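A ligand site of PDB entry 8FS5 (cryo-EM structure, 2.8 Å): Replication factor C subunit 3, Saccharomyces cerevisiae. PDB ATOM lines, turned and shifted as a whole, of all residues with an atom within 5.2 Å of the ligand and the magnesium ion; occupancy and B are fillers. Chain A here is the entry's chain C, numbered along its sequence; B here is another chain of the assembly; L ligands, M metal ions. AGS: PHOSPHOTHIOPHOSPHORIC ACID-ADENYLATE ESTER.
An oxygen (O1B) of the ligand lies within hydrogen-bond range of the backbone NH (N) of Thr 60 (3.2 Å). O2B of the ligand is in hydrogen-bond range of N of Gly 58, 2.5 Å away. The guanidinium group of Arg 183 of chain B sits close to a sulfur (S1G) of the ligand (2.6 Å). The backbone NH of Tyr 28 lies within hydrogen-bond range of a nitrogen (N1) of the ligand. The backbone carbonyl oxygen (O) of Tyr 28 lies within hydrogen-bond range of a nitrogen (N6) of the ligand (2.7 Å). An oxygen (O2A) of the ligand is in salt-bridge range of the guanidinium group (NH2) of Arg 20. N of Thr 57 is in hydrogen-bond range of O2B of the ligand (2.7 Å). S1G of the ligand lies close to NH2 of Arg 206. O3B of the ligand is in hydrogen-bond range of N of Gly 56, 2.8 Å away. O3G of the ligand is in hydrogen-bond range of OD1 of Asn 148 (2.9 Å). N of Lys 59 sits at hydrogen-bond distance from O1B of the ligand. The side-chain amino group of Lys 59 sits at hydrogen-bond distance from an oxygen (O3G) of the ligand (2.9 Å). The backbone NH of Ser 61 sits at hydrogen-bond distance from an oxygen (O1A) of the ligand, 3.2 Å away. The side-chain hydroxyl (OG) of Ser 61 is in hydrogen-bond range of an oxygen (O1A) of the ligand (3.0 Å). An oxygen (O3') of the ligand lies within hydrogen-bond range of the backbone carbonyl oxygen of Val 16 (3.0 Å). The backbone carbonyl oxygen (O) of Tyr 19 sits at hydrogen-bond distance from an oxygen (O2') of the ligand (3.3 Å). S1G of the ligand lies close to NH2 of Arg 154 of chain B (3.6 Å).
OD2 of Asp 117 lies close to OG1 of Thr 60 (3.2 Å). The side-chain carboxylate (OE2) of Glu 158 of chain B lies within salt-bridge range of the guanidinium group (NH1) of Arg 183 of chain B (3.2 Å). The side-chain hydroxyl (OG) of Ser 61 lies within hydrogen-bond range of the guanidinium group (NH1) of Arg 20 (3.1 Å). O of Thr 57 sits at hydrogen-bond distance from NE2 of Gln 30, 3.3 Å away. The guanidinium group of Arg 206 lies within salt-bridge range of the side-chain carboxylate of Glu 158 of chain B, at 2.8 Å. The backbone carbonyl oxygen of Gly 56 is in hydrogen-bond range of the backbone NH of Met 205 (3.5 Å). The side-chain carboxylate of Glu 118 is in salt-bridge range of the guanidinium group of Arg 154 of chain B (3.8 Å). N of Glu 118 sits at hydrogen-bond distance from O of Leu 146, at 3.0 Å.
The backbone carbonyl oxygen (O) of Glu 26 sits close to a nitrogen (N1) of the ligand, at 3.5 Å. O2A of the ligand sits close to OE2 of Glu 158 of chain B (3.4 Å). Residues that only touch the ligand: Pro 55 (3.6 Å), Met 205 (3.6 Å), Val 27 (3.6 Å), Pro 21 (3.7 Å), Leu 209 (3.7 Å), Leu 169 (3.7 Å), Arg 177 (3.9 Å) and Pro 179 of chain B (3.96 Å). Hydrophobic or aromatic side chains within 4 Å of the ligand: Pro 21, Val 27, Pro 55, Leu 169, Met 205, Leu 209 and Pro 179 of chain B.
Asp 117 touches the magnesium ion (OD2 to MG, 3.2 Å). OE2 of Glu 118 touches the magnesium ion (3.9 Å). Three residues have an atom within 4 Å of the magnesium ion: Thr 60, Asp 117 and Glu 118. Along chain A the residues within 4 Å of the magnesium ion span positions 60 to 118. The nearest printed residue that does not touch the magnesium ion is Arg 183 of chain B (4.3 Å).
O2G of the ligand binds the magnesium ion. OG1 of Thr 60 binds the magnesium ion (2.3 Å). The magnesium ion has two donor atoms within binding distance.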
ATOM      1  N   TRP A  15     -17.069  -7.981 -17.436  1.00  0.00           N
ATOM      2  CA  TRP A  15     -18.350  -8.013 -16.745  1.00  0.00           C
ATOM      3  C   TRP A  15     -19.353  -8.921 -17.434  1.00  0.00           C
ATOM      4  O   TRP A  15     -20.255  -9.467 -16.783  1.00  0.00           O
ATOM      5  CB  TRP A  15     -18.906  -6.597 -16.617  1.00  0.00           C
ATOM      6  CG  TRP A  15     -18.164  -5.733 -15.634  1.00  0.00           C
ATOM      7  CD1 TRP A  15     -16.927  -5.964 -15.113  1.00  0.00           C
ATOM      8  CD2 TRP A  15     -18.617  -4.503 -15.069  1.00  0.00           C
ATOM      9  NE1 TRP A  15     -16.579  -4.960 -14.254  1.00  0.00           N
ATOM     10  CE2 TRP A  15     -17.593  -4.040 -14.208  1.00  0.00           C
ATOM     11  CE3 TRP A  15     -19.783  -3.735 -15.201  1.00  0.00           C
ATOM     12  CZ2 TRP A  15     -17.712  -2.853 -13.480  1.00  0.00           C
ATOM     13  CZ3 TRP A  15     -19.890  -2.560 -14.476  1.00  0.00           C
ATOM     14  CH2 TRP A  15     -18.861  -2.131 -13.626  1.00  0.00           C
ATOM     15  N   VAL A  16     -19.224  -9.095 -18.762  1.00  0.00           N
ATOM     16  CA  VAL A  16     -20.096 -10.021 -19.481  1.00  0.00           C
ATOM     17  C   VAL A  16     -19.826 -11.476 -19.126  1.00  0.00           C
ATOM     18  O   VAL A  16     -20.713 -12.320 -19.315  1.00  0.00           O
ATOM     19  CB  VAL A  16     -19.957  -9.829 -21.002  1.00  0.00           C
ATOM     20  CG1 VAL A  16     -20.434  -8.439 -21.403  1.00  0.00           C
ATOM     21  CG2 VAL A  16     -18.519 -10.051 -21.437  1.00  0.00           C
ATOM     22  N   GLU A  17     -18.638 -11.788 -18.615  1.00  0.00           N
ATOM     23  CA  GLU A  17     -18.302 -13.133 -18.162  1.00  0.00           C
ATOM     24  C   GLU A  17     -18.285 -13.280 -16.654  1.00  0.00           C
ATOM     25  O   GLU A  17     -18.537 -14.367 -16.147  1.00  0.00           O
ATOM     26  CB  GLU A  17     -16.941 -13.561 -18.719  1.00  0.00           C
ATOM     27  CG  GLU A  17     -16.779 -13.344 -20.216  1.00  0.00           C
ATOM     28  CD  GLU A  17     -17.427 -14.445 -21.029  1.00  0.00           C
ATOM     29  OE1 GLU A  17     -17.704 -14.204 -22.223  1.00  0.00           O
ATOM     30  OE2 GLU A  17     -17.641 -15.546 -20.479  1.00  0.00           O
ATOM     31  N   TYR A  19     -20.414 -11.802 -14.555  1.00  0.00           N
ATOM     32  CA  TYR A  19     -21.786 -11.846 -14.088  1.00  0.00           C
ATOM     33  C   TYR A  19     -22.630 -12.867 -14.848  1.00  0.00           C
ATOM     34  O   TYR A  19     -23.850 -12.708 -14.963  1.00  0.00           O
ATOM     35  CB  TYR A  19     -22.426 -10.463 -14.176  1.00  0.00           C
ATOM     36  CG  TYR A  19     -21.833  -9.464 -13.202  1.00  0.00           C
ATOM     37  CD1 TYR A  19     -22.239  -9.444 -11.882  1.00  0.00           C
ATOM     38  CD2 TYR A  19     -20.860  -8.561 -13.617  1.00  0.00           C
ATOM     39  CE1 TYR A  19     -21.700  -8.541 -10.983  1.00  0.00           C
ATOM     40  CE2 TYR A  19     -20.318  -7.660 -12.728  1.00  0.00           C
ATOM     41  CZ  TYR A  19     -20.743  -7.650 -11.413  1.00  0.00           C
ATOM     42  OH  TYR A  19     -20.202  -6.758 -10.521  1.00  0.00           O
ATOM     43  N   ARG A  20     -21.992 -13.905 -15.366  1.00  0.00           N
ATOM     44  CA  ARG A  20     -22.740 -14.996 -15.989  1.00  0.00           C
ATOM     45  C   ARG A  20     -23.542 -15.742 -14.920  1.00  0.00           C
ATOM     46  O   ARG A  20     -22.987 -16.092 -13.871  1.00  0.00           O
ATOM     47  CB  ARG A  20     -21.796 -15.960 -16.701  1.00  0.00           C
ATOM     48  CG  ARG A  20     -22.454 -17.239 -17.170  1.00  0.00           C
ATOM     49  CD  ARG A  20     -21.537 -18.046 -18.056  1.00  0.00           C
ATOM     50  NE  ARG A  20     -21.176 -17.305 -19.263  1.00  0.00           N
ATOM     51  CZ  ARG A  20     -21.864 -17.345 -20.398  1.00  0.00           C
ATOM     52  NH1 ARG A  20     -22.952 -18.084 -20.521  1.00  0.00           N
ATOM     53  NH2 ARG A  20     -21.445 -16.620 -21.432  1.00  0.00           N
ATOM     54  N   PRO A  21     -24.833 -15.972 -15.140  1.00  0.00           N
ATOM     55  CA  PRO A  21     -25.637 -16.694 -14.145  1.00  0.00           C
ATOM     56  C   PRO A  21     -25.113 -18.104 -13.908  1.00  0.00           C
ATOM     57  O   PRO A  21     -24.720 -18.806 -14.840  1.00  0.00           O
ATOM     58  CB  PRO A  21     -27.039 -16.707 -14.759  1.00  0.00           C
ATOM     59  CG  PRO A  21     -27.044 -15.526 -15.667  1.00  0.00           C
ATOM     60  CD  PRO A  21     -25.666 -15.479 -16.254  1.00  0.00           C
ATOM     61  N   GLU A  26     -30.910 -16.766 -11.257  1.00  0.00           N
ATOM     62  CA  GLU A  26     -30.230 -15.551 -11.677  1.00  0.00           C
ATOM     63  C   GLU A  26     -30.482 -15.209 -13.145  1.00  0.00           C
ATOM     64  O   GLU A  26     -29.936 -14.214 -13.628  1.00  0.00           O
ATOM     65  CB  GLU A  26     -28.720 -15.682 -11.426  1.00  0.00           C
ATOM     66  CG  GLU A  26     -28.370 -16.085 -10.013  1.00  0.00           C
ATOM     67  CD  GLU A  26     -26.941 -16.600  -9.894  1.00  0.00           C
ATOM     68  OE1 GLU A  26     -26.196 -16.522 -10.887  1.00  0.00           O
ATOM     69  OE2 GLU A  26     -26.577 -17.088  -8.798  1.00  0.00           O
ATOM     70  N   VAL A  27     -31.299 -15.992 -13.845  1.00  0.00           N
ATOM     71  CA  VAL A  27     -31.645 -15.698 -15.239  1.00  0.00           C
ATOM     72  C   VAL A  27     -32.949 -14.915 -15.221  1.00  0.00           C
ATOM     73  O   VAL A  27     -34.000 -15.438 -14.839  1.00  0.00           O
ATOM     74  CB  VAL A  27     -31.776 -16.990 -16.065  1.00  0.00           C
ATOM     75  CG1 VAL A  27     -32.287 -16.671 -17.456  1.00  0.00           C
ATOM     76  CG2 VAL A  27     -30.432 -17.705 -16.129  1.00  0.00           C
ATOM     77  N   TYR A  28     -32.883 -13.660 -15.650  1.00  0.00           N
ATOM     78  CA  TYR A  28     -34.033 -12.768 -15.641  1.00  0.00           C
ATOM     79  C   TYR A  28     -34.580 -12.573 -17.047  1.00  0.00           C
ATOM     80  O   TYR A  28     -33.923 -12.891 -18.050  1.00  0.00           O
ATOM     81  CB  TYR A  28     -33.662 -11.413 -15.033  1.00  0.00           C
ATOM     82  CG  TYR A  28     -32.928 -11.521 -13.717  1.00  0.00           C
ATOM     83  CD1 TYR A  28     -33.452 -12.273 -12.664  1.00  0.00           C
ATOM     84  CD2 TYR A  28     -31.721 -10.865 -13.512  1.00  0.00           C
ATOM     85  CE1 TYR A  28     -32.782 -12.370 -11.456  1.00  0.00           C
ATOM     86  CE2 TYR A  28     -31.047 -10.964 -12.312  1.00  0.00           C
ATOM     87  CZ  TYR A  28     -31.582 -11.711 -11.287  1.00  0.00           C
ATOM     88  OH  TYR A  28     -30.917 -11.811 -10.092  1.00  0.00           O
ATOM     89  N   GLY A  29     -35.787 -12.036 -17.124  1.00  0.00           N
ATOM     90  CA  GLY A  29     -36.421 -11.752 -18.401  1.00  0.00           C
ATOM     91  C   GLY A  29     -37.249 -12.897 -18.932  1.00  0.00           C
ATOM     92  O   GLY A  29     -38.411 -12.713 -19.320  1.00  0.00           O
ATOM     93  N   GLN A  30     -36.669 -14.091 -18.941  1.00  0.00           N
ATOM     94  CA  GLN A  30     -37.335 -15.294 -19.445  1.00  0.00           C
ATOM     95  C   GLN A  30     -37.950 -16.007 -18.251  1.00  0.00           C
ATOM     96  O   GLN A  30     -37.309 -16.839 -17.606  1.00  0.00           O
ATOM     97  CB  GLN A  30     -36.360 -16.181 -20.208  1.00  0.00           C
ATOM     98  CG  GLN A  30     -35.188 -15.431 -20.812  1.00  0.00           C
ATOM     99  CD  GLN A  30     -35.594 -14.616 -22.024  1.00  0.00           C
ATOM    100  OE1 GLN A  30     -36.588 -14.899 -22.675  1.00  0.00           O
ATOM    101  NE2 GLN A  30     -34.809 -13.589 -22.327  1.00  0.00           N
ATOM    102  N   GLY A  53     -33.627 -17.271 -29.901  1.00  0.00           N
ATOM    103  CA  GLY A  53     -33.747 -15.885 -29.517  1.00  0.00           C
ATOM    104  C   GLY A  53     -32.608 -15.026 -30.019  1.00  0.00           C
ATOM    105  O   GLY A  53     -31.658 -15.511 -30.654  1.00  0.00           O
ATOM    106  N   PRO A  54     -32.677 -13.724 -29.758  1.00  0.00           N
ATOM    107  CA  PRO A  54     -31.617 -12.808 -30.174  1.00  0.00           C
ATOM    108  C   PRO A  54     -30.351 -13.051 -29.381  1.00  0.00           C
ATOM    109  O   PRO A  54     -30.383 -13.699 -28.319  1.00  0.00           O
ATOM    110  CB  PRO A  54     -32.210 -11.422 -29.875  1.00  0.00           C
ATOM    111  CG  PRO A  54     -33.676 -11.647 -29.779  1.00  0.00           C
ATOM    112  CD  PRO A  54     -33.832 -13.000 -29.183  1.00  0.00           C
ATOM    113  N   PRO A  55     -29.206 -12.558 -29.861  1.00  0.00           N
ATOM    114  CA  PRO A  55     -27.963 -12.702 -29.094  1.00  0.00           C
ATOM    115  C   PRO A  55     -28.037 -11.974 -27.756  1.00  0.00           C
ATOM    116  O   PRO A  55     -28.698 -10.941 -27.626  1.00  0.00           O
ATOM    117  CB  PRO A  55     -26.907 -12.067 -30.016  1.00  0.00           C
ATOM    118  CG  PRO A  55     -27.490 -12.188 -31.376  1.00  0.00           C
ATOM    119  CD  PRO A  55     -28.966 -11.969 -31.190  1.00  0.00           C
ATOM    120  N   GLY A  56     -27.349 -12.534 -26.763  1.00  0.00           N
ATOM    121  CA  GLY A  56     -27.330 -11.952 -25.438  1.00  0.00           C
ATOM    122  C   GLY A  56     -28.652 -11.978 -24.698  1.00  0.00           C
ATOM    123  O   GLY A  56     -28.975 -11.016 -23.996  1.00  0.00           O
ATOM    124  N   THR A  57     -29.415 -13.059 -24.840  1.00  0.00           N
ATOM    125  CA  THR A  57     -30.679 -13.201 -24.135  1.00  0.00           C
ATOM    126  C   THR A  57     -30.641 -14.197 -22.995  1.00  0.00           C
ATOM    127  O   THR A  57     -31.518 -14.161 -22.132  1.00  0.00           O
ATOM    128  CB  THR A  57     -31.796 -13.621 -25.113  1.00  0.00           C
ATOM    129  OG1 THR A  57     -31.279 -14.581 -26.048  1.00  0.00           O
ATOM    130  CG2 THR A  57     -32.317 -12.414 -25.874  1.00  0.00           C
ATOM    131  N   GLY A  58     -29.641 -15.086 -22.956  1.00  0.00           N
ATOM    132  CA  GLY A  58     -29.497 -15.994 -21.840  1.00  0.00           C
ATOM    133  C   GLY A  58     -29.828 -17.438 -22.151  1.00  0.00           C
ATOM    134  O   GLY A  58     -30.351 -18.152 -21.286  1.00  0.00           O
ATOM    135  N   LYS A  59     -29.536 -17.889 -23.370  1.00  0.00           N
ATOM    136  CA  LYS A  59     -29.793 -19.279 -23.732  1.00  0.00           C
ATOM    137  C   LYS A  59     -28.721 -20.211 -23.183  1.00  0.00           C
ATOM    138  O   LYS A  59     -29.033 -21.218 -22.532  1.00  0.00           O
ATOM    139  CB  LYS A  59     -29.900 -19.414 -25.247  1.00  0.00           C
ATOM    140  CG  LYS A  59     -31.107 -18.722 -25.855  1.00  0.00           C
ATOM    141  CD  LYS A  59     -31.031 -18.729 -27.373  1.00  0.00           C
ATOM    142  CE  LYS A  59     -29.854 -17.901 -27.861  1.00  0.00           C
ATOM    143  NZ  LYS A  59     -29.267 -18.455 -29.109  1.00  0.00           N
ATOM    144  N   THR A  60     -27.453 -19.881 -23.434  1.00  0.00           N
ATOM    145  CA  THR A  60     -26.350 -20.672 -22.887  1.00  0.00           C
ATOM    146  C   THR A  60     -26.307 -20.613 -21.368  1.00  0.00           C
ATOM    147  O   THR A  60     -26.077 -21.646 -20.718  1.00  0.00           O
ATOM    148  CB  THR A  60     -25.012 -20.177 -23.465  1.00  0.00           C
ATOM    149  OG1 THR A  60     -25.067 -20.236 -24.900  1.00  0.00           O
ATOM    150  CG2 THR A  60     -23.862 -21.047 -22.978  1.00  0.00           C
ATOM    151  N   SER A  61     -26.549 -19.439 -20.788  1.00  0.00           N
ATOM    152  CA  SER A  61     -26.599 -19.315 -19.336  1.00  0.00           C
ATOM    153  C   SER A  61     -27.732 -20.155 -18.747  1.00  0.00           C
ATOM    154  O   SER A  61     -27.585 -20.706 -17.647  1.00  0.00           O
ATOM    155  CB  SER A  61     -26.751 -17.850 -18.930  1.00  0.00           C
ATOM    156  OG  SER A  61     -25.706 -17.062 -19.463  1.00  0.00           O
ATOM    157  N   ASP A 117     -24.604 -26.012 -29.004  1.00  0.00           N
ATOM    158  CA  ASP A 117     -24.647 -24.557 -29.097  1.00  0.00           C
ATOM    159  C   ASP A 117     -24.256 -24.121 -30.500  1.00  0.00           C
ATOM    160  O   ASP A 117     -23.415 -24.735 -31.157  1.00  0.00           O
ATOM    161  CB  ASP A 117     -23.705 -23.925 -28.069  1.00  0.00           C
ATOM    162  CG  ASP A 117     -23.997 -22.464 -27.822  1.00  0.00           C
ATOM    163  OD1 ASP A 117     -24.924 -21.928 -28.473  1.00  0.00           O
ATOM    164  OD2 ASP A 117     -23.310 -21.845 -26.986  1.00  0.00           O
ATOM    165  N   GLU A 118     -24.902 -23.040 -30.957  1.00  0.00           N
ATOM    166  CA  GLU A 118     -24.673 -22.470 -32.285  1.00  0.00           C
ATOM    167  C   GLU A 118     -24.881 -23.518 -33.375  1.00  0.00           C
ATOM    168  O   GLU A 118     -24.065 -23.676 -34.298  1.00  0.00           O
ATOM    169  CB  GLU A 118     -23.276 -21.848 -32.382  1.00  0.00           C
ATOM    170  CG  GLU A 118     -23.108 -20.611 -31.514  1.00  0.00           C
ATOM    171  CD  GLU A 118     -21.940 -20.707 -30.567  1.00  0.00           C
ATOM    172  OE1 GLU A 118     -20.983 -21.456 -30.873  1.00  0.00           O
ATOM    173  OE2 GLU A 118     -21.973 -20.038 -29.510  1.00  0.00           O
ATOM    174  N   LEU A 146     -29.209 -24.845 -29.336  1.00  0.00           N
ATOM    175  CA  LEU A 146     -29.211 -23.405 -29.162  1.00  0.00           C
ATOM    176  C   LEU A 146     -28.930 -22.752 -30.513  1.00  0.00           C
ATOM    177  O   LEU A 146     -27.930 -23.081 -31.169  1.00  0.00           O
ATOM    178  CB  LEU A 146     -28.156 -22.959 -28.139  1.00  0.00           C
ATOM    179  CG  LEU A 146     -27.985 -23.815 -26.881  1.00  0.00           C
ATOM    180  CD1 LEU A 146     -26.923 -23.214 -25.985  1.00  0.00           C
ATOM    181  CD2 LEU A 146     -29.299 -23.943 -26.133  1.00  0.00           C
ATOM    182  N   ASN A 148     -29.660 -18.938 -33.037  1.00  0.00           N
ATOM    183  CA  ASN A 148     -30.160 -17.580 -33.227  1.00  0.00           C
ATOM    184  C   ASN A 148     -30.912 -17.395 -34.527  1.00  0.00           C
ATOM    185  O   ASN A 148     -31.699 -16.448 -34.639  1.00  0.00           O
ATOM    186  CB  ASN A 148     -29.001 -16.576 -33.179  1.00  0.00           C
ATOM    187  CG  ASN A 148     -28.316 -16.526 -31.826  1.00  0.00           C
ATOM    188  OD1 ASN A 148     -27.193 -17.009 -31.676  1.00  0.00           O
ATOM    189  ND2 ASN A 148     -28.989 -15.944 -30.844  1.00  0.00           N
ATOM    190  N   LEU A 169     -34.772  -8.999 -23.667  1.00  0.00           N
ATOM    191  CA  LEU A 169     -34.890  -8.782 -22.235  1.00  0.00           C
ATOM    192  C   LEU A 169     -35.761  -7.560 -21.942  1.00  0.00           C
ATOM    193  O   LEU A 169     -35.498  -6.480 -22.476  1.00  0.00           O
ATOM    194  CB  LEU A 169     -33.503  -8.602 -21.616  1.00  0.00           C
ATOM    195  CG  LEU A 169     -32.740  -9.898 -21.333  1.00  0.00           C
ATOM    196  CD1 LEU A 169     -31.263  -9.739 -21.664  1.00  0.00           C
ATOM    197  CD2 LEU A 169     -32.940 -10.332 -19.895  1.00  0.00           C
ATOM    198  N   ARG A 177     -31.040  -6.622 -12.997  1.00  0.00           N
ATOM    199  CA  ARG A 177     -29.639  -6.987 -13.130  1.00  0.00           C
ATOM    200  C   ARG A 177     -28.700  -5.803 -12.921  1.00  0.00           C
ATOM    201  O   ARG A 177     -27.624  -5.973 -12.327  1.00  0.00           O
ATOM    202  CB  ARG A 177     -29.377  -7.606 -14.507  1.00  0.00           C
ATOM    203  CG  ARG A 177     -28.075  -8.375 -14.597  1.00  0.00           C
ATOM    204  CD  ARG A 177     -28.015  -9.463 -13.535  1.00  0.00           C
ATOM    205  NE  ARG A 177     -26.782 -10.245 -13.617  1.00  0.00           N
ATOM    206  CZ  ARG A 177     -26.522 -11.306 -12.857  1.00  0.00           C
ATOM    207  NH1 ARG A 177     -27.388 -11.735 -11.955  1.00  0.00           N
ATOM    208  NH2 ARG A 177     -25.369 -11.944 -13.011  1.00  0.00           N
ATOM    209  N   MET A 205     -28.220  -7.985 -22.502  1.00  0.00           N
ATOM    210  CA  MET A 205     -27.498  -7.817 -21.243  1.00  0.00           C
ATOM    211  C   MET A 205     -26.005  -7.626 -21.430  1.00  0.00           C
ATOM    212  O   MET A 205     -25.375  -6.910 -20.644  1.00  0.00           O
ATOM    213  CB  MET A 205     -27.755  -9.015 -20.328  1.00  0.00           C
ATOM    214  CG  MET A 205     -27.765  -8.683 -18.848  1.00  0.00           C
ATOM    215  SD  MET A 205     -29.251  -7.787 -18.366  1.00  0.00           S
ATOM    216  CE  MET A 205     -30.247  -9.125 -17.700  1.00  0.00           C
ATOM    217  N   ARG A 206     -25.430  -8.253 -22.463  1.00  0.00           N
ATOM    218  CA  ARG A 206     -24.004  -8.103 -22.723  1.00  0.00           C
ATOM    219  C   ARG A 206     -23.639  -6.664 -23.044  1.00  0.00           C
ATOM    220  O   ARG A 206     -22.620  -6.155 -22.565  1.00  0.00           O
ATOM    221  CB  ARG A 206     -23.587  -9.030 -23.864  1.00  0.00           C
ATOM    222  CG  ARG A 206     -22.898 -10.306 -23.428  1.00  0.00           C
ATOM    223  CD  ARG A 206     -22.225 -10.992 -24.593  1.00  0.00           C
ATOM    224  NE  ARG A 206     -23.198 -11.457 -25.577  1.00  0.00           N
ATOM    225  CZ  ARG A 206     -23.361 -12.720 -25.934  1.00  0.00           C
ATOM    226  NH1 ARG A 206     -22.633 -13.692 -25.417  1.00  0.00           N
ATOM    227  NH2 ARG A 206     -24.295 -13.024 -26.833  1.00  0.00           N
ATOM    228  N   LEU A 209     -23.739  -4.646 -19.741  1.00  0.00           N
ATOM    229  CA  LEU A 209     -22.525  -4.855 -18.956  1.00  0.00           C
ATOM    230  C   LEU A 209     -21.304  -4.194 -19.571  1.00  0.00           C
ATOM    231  O   LEU A 209     -20.508  -3.589 -18.843  1.00  0.00           O
ATOM    232  CB  LEU A 209     -22.273  -6.347 -18.766  1.00  0.00           C
ATOM    233  CG  LEU A 209     -23.314  -7.069 -17.903  1.00  0.00           C
ATOM    234  CD1 LEU A 209     -23.219  -8.576 -18.065  1.00  0.00           C
ATOM    235  CD2 LEU A 209     -23.157  -6.681 -16.435  1.00  0.00           C
ATOM    236  N   ARG B 154     -17.077 -17.248 -31.247  1.00  0.00           N
ATOM    237  CA  ARG B 154     -17.898 -16.798 -30.136  1.00  0.00           C
ATOM    238  C   ARG B 154     -17.592 -17.571 -28.866  1.00  0.00           C
ATOM    239  O   ARG B 154     -17.274 -16.985 -27.819  1.00  0.00           O
ATOM    240  CB  ARG B 154     -19.380 -16.939 -30.526  1.00  0.00           C
ATOM    241  CG  ARG B 154     -19.725 -16.186 -31.807  1.00  0.00           C
ATOM    242  CD  ARG B 154     -20.910 -16.811 -32.536  1.00  0.00           C
ATOM    243  NE  ARG B 154     -22.095 -16.921 -31.707  1.00  0.00           N
ATOM    244  CZ  ARG B 154     -23.303 -17.262 -32.152  1.00  0.00           C
ATOM    245  NH1 ARG B 154     -23.504 -17.521 -33.439  1.00  0.00           N
ATOM    246  NH2 ARG B 154     -24.313 -17.331 -31.305  1.00  0.00           N
ATOM    247  N   ARG B 155     -17.646 -18.901 -28.936  1.00  0.00           N
ATOM    248  CA  ARG B 155     -17.363 -19.715 -27.765  1.00  0.00           C
ATOM    249  C   ARG B 155     -15.871 -19.746 -27.447  1.00  0.00           C
ATOM    250  O   ARG B 155     -15.496 -20.009 -26.307  1.00  0.00           O
ATOM    251  CB  ARG B 155     -17.896 -21.125 -27.957  1.00  0.00           C
ATOM    252  CG  ARG B 155     -19.418 -21.202 -27.912  1.00  0.00           C
ATOM    253  CD  ARG B 155     -19.967 -20.677 -26.597  1.00  0.00           C
ATOM    254  NE  ARG B 155     -19.458 -21.413 -25.452  1.00  0.00           N
ATOM    255  CZ  ARG B 155     -19.723 -21.110 -24.193  1.00  0.00           C
ATOM    256  NH1 ARG B 155     -20.484 -20.076 -23.871  1.00  0.00           N
ATOM    257  NH2 ARG B 155     -19.207 -21.856 -23.222  1.00  0.00           N
ATOM    258  N   GLU B 158     -15.696 -16.678 -25.336  1.00  0.00           N
ATOM    259  CA  GLU B 158     -16.429 -16.832 -24.083  1.00  0.00           C
ATOM    260  C   GLU B 158     -15.780 -17.826 -23.113  1.00  0.00           C
ATOM    261  O   GLU B 158     -15.705 -17.555 -21.915  1.00  0.00           O
ATOM    262  CB  GLU B 158     -17.873 -17.255 -24.348  1.00  0.00           C
ATOM    263  CG  GLU B 158     -18.797 -16.101 -24.683  1.00  0.00           C
ATOM    264  CD  GLU B 158     -20.235 -16.398 -24.311  1.00  0.00           C
ATOM    265  OE1 GLU B 158     -20.633 -17.587 -24.339  1.00  0.00           O
ATOM    266  OE2 GLU B 158     -20.973 -15.439 -23.993  1.00  0.00           O
ATOM    267  N   PRO B 179     -23.731 -11.610 -33.076  1.00  0.00           N
ATOM    268  CA  PRO B 179     -23.234 -12.349 -31.903  1.00  0.00           C
ATOM    269  C   PRO B 179     -21.824 -11.957 -31.476  1.00  0.00           C
ATOM    270  O   PRO B 179     -21.556 -11.886 -30.268  1.00  0.00           O
ATOM    271  CB  PRO B 179     -23.297 -13.810 -32.366  1.00  0.00           C
ATOM    272  CG  PRO B 179     -24.422 -13.830 -33.309  1.00  0.00           C
ATOM    273  CD  PRO B 179     -24.304 -12.534 -34.073  1.00  0.00           C
ATOM    274  N   ARG B 183     -20.572  -9.566 -27.843  1.00  0.00           N
ATOM    275  CA  ARG B 183     -19.562  -9.993 -26.873  1.00  0.00           C
ATOM    276  C   ARG B 183     -18.369  -9.036 -26.799  1.00  0.00           C
ATOM    277  O   ARG B 183     -17.593  -9.129 -25.848  1.00  0.00           O
ATOM    278  CB  ARG B 183     -19.067 -11.392 -27.221  1.00  0.00           C
ATOM    279  CG  ARG B 183     -20.188 -12.397 -27.387  1.00  0.00           C
ATOM    280  CD  ARG B 183     -19.724 -13.653 -28.108  1.00  0.00           C
ATOM    281  NE  ARG B 183     -20.833 -14.313 -28.785  1.00  0.00           N
ATOM    282  CZ  ARG B 183     -21.459 -15.387 -28.314  1.00  0.00           C
ATOM    283  NH1 ARG B 183     -21.097 -15.960 -27.185  1.00  0.00           N
ATOM    284  NH2 ARG B 183     -22.481 -15.891 -28.996  1.00  0.00           N
HETATM  285  PG  AGS L   1     -25.953 -16.029 -27.873  1.00  0.00           P
HETATM  286  S1G AGS L   1     -24.858 -14.741 -28.853  1.00  0.00           S
HETATM  287  O2G AGS L   1     -25.048 -17.158 -27.307  1.00  0.00           O
HETATM  288  O3G AGS L   1     -26.994 -16.649 -28.844  1.00  0.00           O
HETATM  289  PB  AGS L   1     -26.751 -15.976 -25.263  1.00  0.00           P
HETATM  290  O1B AGS L   1     -27.232 -17.371 -25.371  1.00  0.00           O
HETATM  291  O2B AGS L   1     -27.671 -15.086 -24.422  1.00  0.00           O
HETATM  292  O3B AGS L   1     -26.690 -15.306 -26.710  1.00  0.00           O
HETATM  293  PA  AGS L   1     -25.212 -15.942 -22.992  1.00  0.00           P
HETATM  294  O1A AGS L   1     -26.348 -16.660 -22.370  1.00  0.00           O
HETATM  295  O2A AGS L   1     -23.848 -16.547 -22.664  1.00  0.00           O
HETATM  296  O3A AGS L   1     -25.327 -15.926 -24.572  1.00  0.00           O
HETATM  297  O5' AGS L   1     -25.288 -14.419 -22.536  1.00  0.00           O
HETATM  298  C5' AGS L   1     -24.088 -13.625 -22.449  1.00  0.00           C
HETATM  299  C4' AGS L   1     -24.016 -12.969 -21.098  1.00  0.00           C
HETATM  300  O4' AGS L   1     -25.118 -12.047 -20.944  1.00  0.00           O
HETATM  301  C3' AGS L   1     -24.118 -13.911 -19.909  1.00  0.00           C
HETATM  302  O3' AGS L   1     -22.855 -14.454 -19.572  1.00  0.00           O
HETATM  303  C2' AGS L   1     -24.647 -12.995 -18.811  1.00  0.00           C
HETATM  304  O2' AGS L   1     -23.598 -12.277 -18.175  1.00  0.00           O
HETATM  305  C1' AGS L   1     -25.555 -12.040 -19.599  1.00  0.00           C
HETATM  306  N9  AGS L   1     -26.967 -12.409 -19.576  1.00  0.00           N
HETATM  307  C8  AGS L   1     -27.735 -12.806 -20.638  1.00  0.00           C
HETATM  308  N7  AGS L   1     -28.982 -13.075 -20.338  1.00  0.00           N
HETATM  309  C5  AGS L   1     -29.031 -12.847 -18.969  1.00  0.00           C
HETATM  310  C6  AGS L   1     -30.088 -12.953 -18.032  1.00  0.00           C
HETATM  311  N6  AGS L   1     -31.319 -13.333 -18.343  1.00  0.00           N
HETATM  312  N1  AGS L   1     -29.802 -12.649 -16.744  1.00  0.00           N
HETATM  313  C2  AGS L   1     -28.566 -12.266 -16.420  1.00  0.00           C
HETATM  314  N3  AGS L   1     -27.501 -12.128 -17.219  1.00  0.00           N
HETATM  315  C4  AGS L   1     -27.809 -12.435 -18.481  1.00  0.00           C
HETATM  316 MG    MG M   1     -24.231 -18.871 -26.488  1.00  0.00          MG
